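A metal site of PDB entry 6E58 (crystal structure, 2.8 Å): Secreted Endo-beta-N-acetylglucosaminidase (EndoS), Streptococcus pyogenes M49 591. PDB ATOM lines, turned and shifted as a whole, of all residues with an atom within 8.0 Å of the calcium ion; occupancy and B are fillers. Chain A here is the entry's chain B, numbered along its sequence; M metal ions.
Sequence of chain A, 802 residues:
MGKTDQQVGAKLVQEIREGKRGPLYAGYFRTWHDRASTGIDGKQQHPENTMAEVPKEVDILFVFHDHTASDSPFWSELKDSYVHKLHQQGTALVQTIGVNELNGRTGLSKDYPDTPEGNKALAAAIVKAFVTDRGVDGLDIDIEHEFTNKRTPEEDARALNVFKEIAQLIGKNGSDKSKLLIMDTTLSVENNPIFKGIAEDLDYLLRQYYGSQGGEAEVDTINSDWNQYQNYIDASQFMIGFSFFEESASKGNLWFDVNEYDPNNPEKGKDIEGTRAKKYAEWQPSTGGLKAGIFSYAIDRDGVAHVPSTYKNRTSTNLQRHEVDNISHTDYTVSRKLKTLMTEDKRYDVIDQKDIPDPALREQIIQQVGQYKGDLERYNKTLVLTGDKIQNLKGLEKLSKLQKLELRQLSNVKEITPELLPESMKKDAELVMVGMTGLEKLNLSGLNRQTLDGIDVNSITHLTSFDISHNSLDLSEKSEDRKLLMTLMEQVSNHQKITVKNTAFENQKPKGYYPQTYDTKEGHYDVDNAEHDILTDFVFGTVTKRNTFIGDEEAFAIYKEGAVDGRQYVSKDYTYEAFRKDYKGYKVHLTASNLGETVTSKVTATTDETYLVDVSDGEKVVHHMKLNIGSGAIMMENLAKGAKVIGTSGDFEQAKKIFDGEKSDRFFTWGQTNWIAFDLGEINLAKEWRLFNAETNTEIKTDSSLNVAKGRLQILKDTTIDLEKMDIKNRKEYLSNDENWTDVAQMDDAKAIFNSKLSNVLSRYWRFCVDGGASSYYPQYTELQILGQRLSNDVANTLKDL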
ATOM      1  N   GLN A 654     -12.550  13.157 -13.118  1.00  0.00           N
ATOM      2  CA  GLN A 654     -13.850  12.509 -12.992  1.00  0.00           C
ATOM      3  C   GLN A 654     -13.739  11.266 -12.119  1.00  0.00           C
ATOM      4  O   GLN A 654     -14.727  10.867 -11.484  1.00  0.00           O
ATOM      5  CB  GLN A 654     -14.415  12.101 -14.339  1.00  0.00           C
ATOM      6  CG  GLN A 654     -14.798  13.212 -15.290  1.00  0.00           C
ATOM      7  CD  GLN A 654     -14.916  12.691 -16.730  1.00  0.00           C
ATOM      8  OE1 GLN A 654     -15.470  11.602 -16.977  1.00  0.00           O
ATOM      9  NE2 GLN A 654     -14.365  13.461 -17.691  1.00  0.00           N
ATOM     10  N   ALA A 655     -12.568  10.617 -12.104  1.00  0.00           N
ATOM     11  CA  ALA A 655     -12.357   9.500 -11.187  1.00  0.00           C
ATOM     12  C   ALA A 655     -12.504   9.924  -9.739  1.00  0.00           C
ATOM     13  O   ALA A 655     -13.036   9.174  -8.906  1.00  0.00           O
ATOM     14  CB  ALA A 655     -10.985   8.871 -11.422  1.00  0.00           C
ATOM     15  N   LYS A 656     -12.038  11.134  -9.394  1.00  0.00           N
ATOM     16  CA  LYS A 656     -12.059  11.579  -8.010  1.00  0.00           C
ATOM     17  C   LYS A 656     -13.472  11.754  -7.477  1.00  0.00           C
ATOM     18  O   LYS A 656     -13.674  11.654  -6.268  1.00  0.00           O
ATOM     19  CB  LYS A 656     -11.362  12.925  -7.865  1.00  0.00           C
ATOM     20  CG  LYS A 656      -9.872  12.948  -8.015  1.00  0.00           C
ATOM     21  CD  LYS A 656      -9.390  14.382  -7.858  1.00  0.00           C
ATOM     22  CE  LYS A 656      -7.887  14.432  -7.678  1.00  0.00           C
ATOM     23  NZ  LYS A 656      -7.371  15.815  -7.926  1.00  0.00           N
ATOM     24  N   LYS A 657     -14.454  11.951  -8.336  1.00  0.00           N
ATOM     25  CA  LYS A 657     -15.796  12.227  -7.847  1.00  0.00           C
ATOM     26  C   LYS A 657     -16.568  10.960  -7.528  1.00  0.00           C
ATOM     27  O   LYS A 657     -17.742  11.065  -7.172  1.00  0.00           O
ATOM     28  CB  LYS A 657     -16.561  13.077  -8.869  1.00  0.00           C
ATOM     29  CG  LYS A 657     -16.066  14.515  -9.011  1.00  0.00           C
ATOM     30  CD  LYS A 657     -16.965  15.466  -9.849  1.00  0.00           C
ATOM     31  CE  LYS A 657     -16.920  15.199 -11.332  1.00  0.00           C
ATOM     32  NZ  LYS A 657     -17.308  13.879 -11.827  1.00  0.00           N
ATOM     33  N   ILE A 658     -15.963   9.774  -7.573  1.00  0.00           N
ATOM     34  CA  ILE A 658     -16.668   8.577  -7.108  1.00  0.00           C
ATOM     35  C   ILE A 658     -16.293   8.296  -5.672  1.00  0.00           C
ATOM     36  O   ILE A 658     -16.703   7.276  -5.096  1.00  0.00           O
ATOM     37  CB  ILE A 658     -16.389   7.339  -7.983  1.00  0.00           C
ATOM     38  CG1 ILE A 658     -15.013   6.762  -7.636  1.00  0.00           C
ATOM     39  CG2 ILE A 658     -16.543   7.684  -9.459  1.00  0.00           C
ATOM     40  CD1 ILE A 658     -14.808   5.358  -8.126  1.00  0.00           C
ATOM     41  N   PHE A 659     -15.522   9.201  -5.075  1.00  0.00           N
ATOM     42  CA  PHE A 659     -15.113   9.028  -3.684  1.00  0.00           C
ATOM     43  C   PHE A 659     -15.463  10.237  -2.825  1.00  0.00           C
ATOM     44  O   PHE A 659     -14.835  10.457  -1.794  1.00  0.00           O
ATOM     45  CB  PHE A 659     -13.606   8.729  -3.573  1.00  0.00           C
ATOM     46  CG  PHE A 659     -13.160   7.489  -4.302  1.00  0.00           C
ATOM     47  CD1 PHE A 659     -12.029   7.506  -5.077  1.00  0.00           C
ATOM     48  CD2 PHE A 659     -13.827   6.286  -4.129  1.00  0.00           C
ATOM     49  CE1 PHE A 659     -11.615   6.352  -5.731  1.00  0.00           C
ATOM     50  CE2 PHE A 659     -13.422   5.123  -4.789  1.00  0.00           C
ATOM     51  CZ  PHE A 659     -12.313   5.167  -5.586  1.00  0.00           C
ATOM     52  N   ASP A 660     -16.422  11.057  -3.251  1.00  0.00           N
ATOM     53  CA  ASP A 660     -16.982  12.086  -2.380  1.00  0.00           C
ATOM     54  C   ASP A 660     -18.247  11.505  -1.727  1.00  0.00           C
ATOM     55  O   ASP A 660     -18.445  10.292  -1.730  1.00  0.00           O
ATOM     56  CB  ASP A 660     -17.200  13.384  -3.177  1.00  0.00           C
ATOM     57  CG  ASP A 660     -18.117  13.198  -4.373  1.00  0.00           C
ATOM     58  OD1 ASP A 660     -18.928  12.241  -4.385  1.00  0.00           O
ATOM     59  OD2 ASP A 660     -18.015  14.010  -5.321  1.00  0.00           O
ATOM     60  N   GLY A 661     -19.134  12.347  -1.192  1.00  0.00           N
ATOM     61  CA  GLY A 661     -20.291  11.803  -0.512  1.00  0.00           C
ATOM     62  C   GLY A 661     -21.482  11.564  -1.426  1.00  0.00           C
ATOM     63  O   GLY A 661     -22.339  10.707  -1.154  1.00  0.00           O
ATOM     64  N   GLU A 662     -21.514  12.291  -2.525  1.00  0.00           N
ATOM     65  CA  GLU A 662     -22.731  12.495  -3.289  1.00  0.00           C
ATOM     66  C   GLU A 662     -22.817  11.493  -4.438  1.00  0.00           C
ATOM     67  O   GLU A 662     -21.882  10.749  -4.734  1.00  0.00           O
ATOM     68  CB  GLU A 662     -22.773  13.939  -3.821  1.00  0.00           C
ATOM     69  N   LYS A 663     -23.988  11.455  -5.051  1.00  0.00           N
ATOM     70  CA  LYS A 663     -24.242  10.748  -6.301  1.00  0.00           C
ATOM     71  C   LYS A 663     -24.672  11.720  -7.398  1.00  0.00           C
ATOM     72  O   LYS A 663     -25.560  11.435  -8.202  1.00  0.00           O
ATOM     73  CB  LYS A 663     -25.260   9.622  -6.105  1.00  0.00           C
ATOM     74  CG  LYS A 663     -24.909   8.711  -4.938  1.00  0.00           C
ATOM     75  CD  LYS A 663     -25.635   9.001  -3.652  1.00  0.00           C
ATOM     76  CE  LYS A 663     -25.462   7.839  -2.678  1.00  0.00           C
ATOM     77  NZ  LYS A 663     -26.610   7.692  -1.716  1.00  0.00           N
ATOM     78  N   SER A 664     -24.034  12.883  -7.413  1.00  0.00           N
ATOM     79  CA  SER A 664     -24.326  13.995  -8.327  1.00  0.00           C
ATOM     80  C   SER A 664     -23.337  14.057  -9.483  1.00  0.00           C
ATOM     81  O   SER A 664     -22.910  15.127  -9.907  1.00  0.00           O
ATOM     82  CB  SER A 664     -24.329  15.309  -7.549  1.00  0.00           C
ATOM     83  OG  SER A 664     -23.066  15.518  -6.912  1.00  0.00           O
ATOM     84  N   ASP A 665     -22.964  12.909 -10.031  1.00  0.00           N
ATOM     85  CA  ASP A 665     -21.816  12.844 -10.931  1.00  0.00           C
ATOM     86  C   ASP A 665     -21.764  11.463 -11.550  1.00  0.00           C
ATOM     87  O   ASP A 665     -22.514  10.560 -11.180  1.00  0.00           O
ATOM     88  CB  ASP A 665     -20.544  13.117 -10.148  1.00  0.00           C
ATOM     89  CG  ASP A 665     -20.500  12.317  -8.856  1.00  0.00           C
ATOM     90  OD1 ASP A 665     -20.339  11.086  -8.936  1.00  0.00           O
ATOM     91  OD2 ASP A 665     -20.718  12.916  -7.776  1.00  0.00           O
ATOM     92  N   ARG A 666     -20.845  11.292 -12.487  1.00  0.00           N
ATOM     93  CA  ARG A 666     -20.757  10.006 -13.152  1.00  0.00           C
ATOM     94  C   ARG A 666     -19.332   9.845 -13.658  1.00  0.00           C
ATOM     95  O   ARG A 666     -18.648  10.827 -13.955  1.00  0.00           O
ATOM     96  CB  ARG A 666     -21.762   9.904 -14.297  1.00  0.00           C
ATOM     97  CG  ARG A 666     -21.627  11.021 -15.292  1.00  0.00           C
ATOM     98  CD  ARG A 666     -22.763  11.023 -16.278  1.00  0.00           C
ATOM     99  NE  ARG A 666     -22.521  12.077 -17.267  1.00  0.00           N
ATOM    100  CZ  ARG A 666     -23.332  12.338 -18.277  1.00  0.00           C
ATOM    101  NH1 ARG A 666     -24.458  11.652 -18.406  1.00  0.00           N
ATOM    102  NH2 ARG A 666     -23.028  13.282 -19.150  1.00  0.00           N
ATOM    103  N   PHE A 692     -22.813   2.387  -6.230  1.00  0.00           N
ATOM    104  CA  PHE A 692     -24.007   3.097  -6.676  1.00  0.00           C
ATOM    105  C   PHE A 692     -23.936   3.213  -8.191  1.00  0.00           C
ATOM    106  O   PHE A 692     -23.036   3.872  -8.731  1.00  0.00           O
ATOM    107  CB  PHE A 692     -24.109   4.465  -5.991  1.00  0.00           C
ATOM    108  CG  PHE A 692     -24.256   4.398  -4.478  1.00  0.00           C
ATOM    109  CD1 PHE A 692     -25.464   4.072  -3.886  1.00  0.00           C
ATOM    110  CD2 PHE A 692     -23.161   4.648  -3.646  1.00  0.00           C
ATOM    111  CE1 PHE A 692     -25.581   4.007  -2.507  1.00  0.00           C
ATOM    112  CE2 PHE A 692     -23.286   4.587  -2.263  1.00  0.00           C
ATOM    113  CZ  PHE A 692     -24.492   4.264  -1.695  1.00  0.00           C
ATOM    114  N   TYR A 781     -21.099   5.024 -13.485  1.00  0.00           N
ATOM    115  CA  TYR A 781     -21.434   4.805 -12.089  1.00  0.00           C
ATOM    116  C   TYR A 781     -21.073   6.045 -11.297  1.00  0.00           C
ATOM    117  O   TYR A 781     -20.238   6.851 -11.729  1.00  0.00           O
ATOM    118  CB  TYR A 781     -20.769   3.535 -11.527  1.00  0.00           C
ATOM    119  CG  TYR A 781     -19.259   3.472 -11.478  1.00  0.00           C
ATOM    120  CD1 TYR A 781     -18.541   3.003 -12.570  1.00  0.00           C
ATOM    121  CD2 TYR A 781     -18.551   3.791 -10.333  1.00  0.00           C
ATOM    122  CE1 TYR A 781     -17.166   2.910 -12.532  1.00  0.00           C
ATOM    123  CE2 TYR A 781     -17.158   3.693 -10.283  1.00  0.00           C
ATOM    124  CZ  TYR A 781     -16.473   3.248 -11.390  1.00  0.00           C
ATOM    125  OH  TYR A 781     -15.099   3.144 -11.387  1.00  0.00           O
ATOM    126  N   THR A 782     -21.722   6.222 -10.138  1.00  0.00           N
ATOM    127  CA  THR A 782     -21.661   7.484  -9.421  1.00  0.00           C
ATOM    128  C   THR A 782     -20.865   7.447  -8.126  1.00  0.00           C
ATOM    129  O   THR A 782     -20.275   8.464  -7.760  1.00  0.00           O
ATOM    130  CB  THR A 782     -23.080   7.991  -9.099  1.00  0.00           C
ATOM    131  OG1 THR A 782     -23.655   7.171  -8.076  1.00  0.00           O
ATOM    132  CG2 THR A 782     -23.947   7.925 -10.351  1.00  0.00           C
ATOM    133  N   GLU A 783     -20.804   6.315  -7.423  1.00  0.00           N
ATOM    134  CA  GLU A 783     -20.144   6.277  -6.127  1.00  0.00           C
ATOM    135  C   GLU A 783     -19.748   4.855  -5.775  1.00  0.00           C
ATOM    136  O   GLU A 783     -20.498   3.914  -6.045  1.00  0.00           O
ATOM    137  CB  GLU A 783     -21.033   6.863  -5.005  1.00  0.00           C
ATOM    138  CG  GLU A 783     -20.422   6.773  -3.620  1.00  0.00           C
ATOM    139  CD  GLU A 783     -19.501   7.933  -3.269  1.00  0.00           C
ATOM    140  OE1 GLU A 783     -19.475   8.929  -4.010  1.00  0.00           O
ATOM    141  OE2 GLU A 783     -18.770   7.823  -2.272  1.00  0.00           O
ATOM    142  N   LEU A 784     -18.573   4.710  -5.149  1.00  0.00           N
ATOM    143  CA  LEU A 784     -18.029   3.431  -4.735  1.00  0.00           C
ATOM    144  C   LEU A 784     -17.722   3.500  -3.251  1.00  0.00           C
ATOM    145  O   LEU A 784     -17.140   4.482  -2.787  1.00  0.00           O
ATOM    146  CB  LEU A 784     -16.765   3.095  -5.538  1.00  0.00           C
ATOM    147  CG  LEU A 784     -16.207   1.681  -5.423  1.00  0.00           C
ATOM    148  CD1 LEU A 784     -17.065   0.708  -6.224  1.00  0.00           C
ATOM    149  CD2 LEU A 784     -14.770   1.654  -5.926  1.00  0.00           C
HETATM  150 CA    CA M   1     -19.765  10.513  -5.783  1.00  0.00          CA
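The backbone carbonyl oxygen of Ile 658 sits at hydrogen-bond distance from the backbone NH of Leu 784 (3.2 Å).
O of Glu 783 sits at hydrogen-bond distance from N of Phe 692.
The backbone NH of Thr 782 is in hydrogen-bond range of the backbone carbonyl oxygen of Phe 692 (3.0 Å).
The calcium ion is bound by O of Glu 662 (2.4 Å).
The calcium ion is bound by the side-chain carboxylate (OD1) of Asp 660, 2.4 Å away.
OE1 of Glu 783 is bound to the calcium ion (2.4 Å).
O of Lys 657 binds the calcium ion, at 2.5 Å.
The calcium ion is bound by O of Thr 782.
The calcium ion has five donor atoms within binding distance.
Ile 658 touches the calcium ion (CA to CA, 3.9 Å).
Asp 665 touches the calcium ion (OD1 to CA, 3.3 Å).
Within 4 Å of the calcium ion: Lys 657, Ile 658, Asp 660, Glu 662, Asp 665, Thr 782 and Glu 783.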
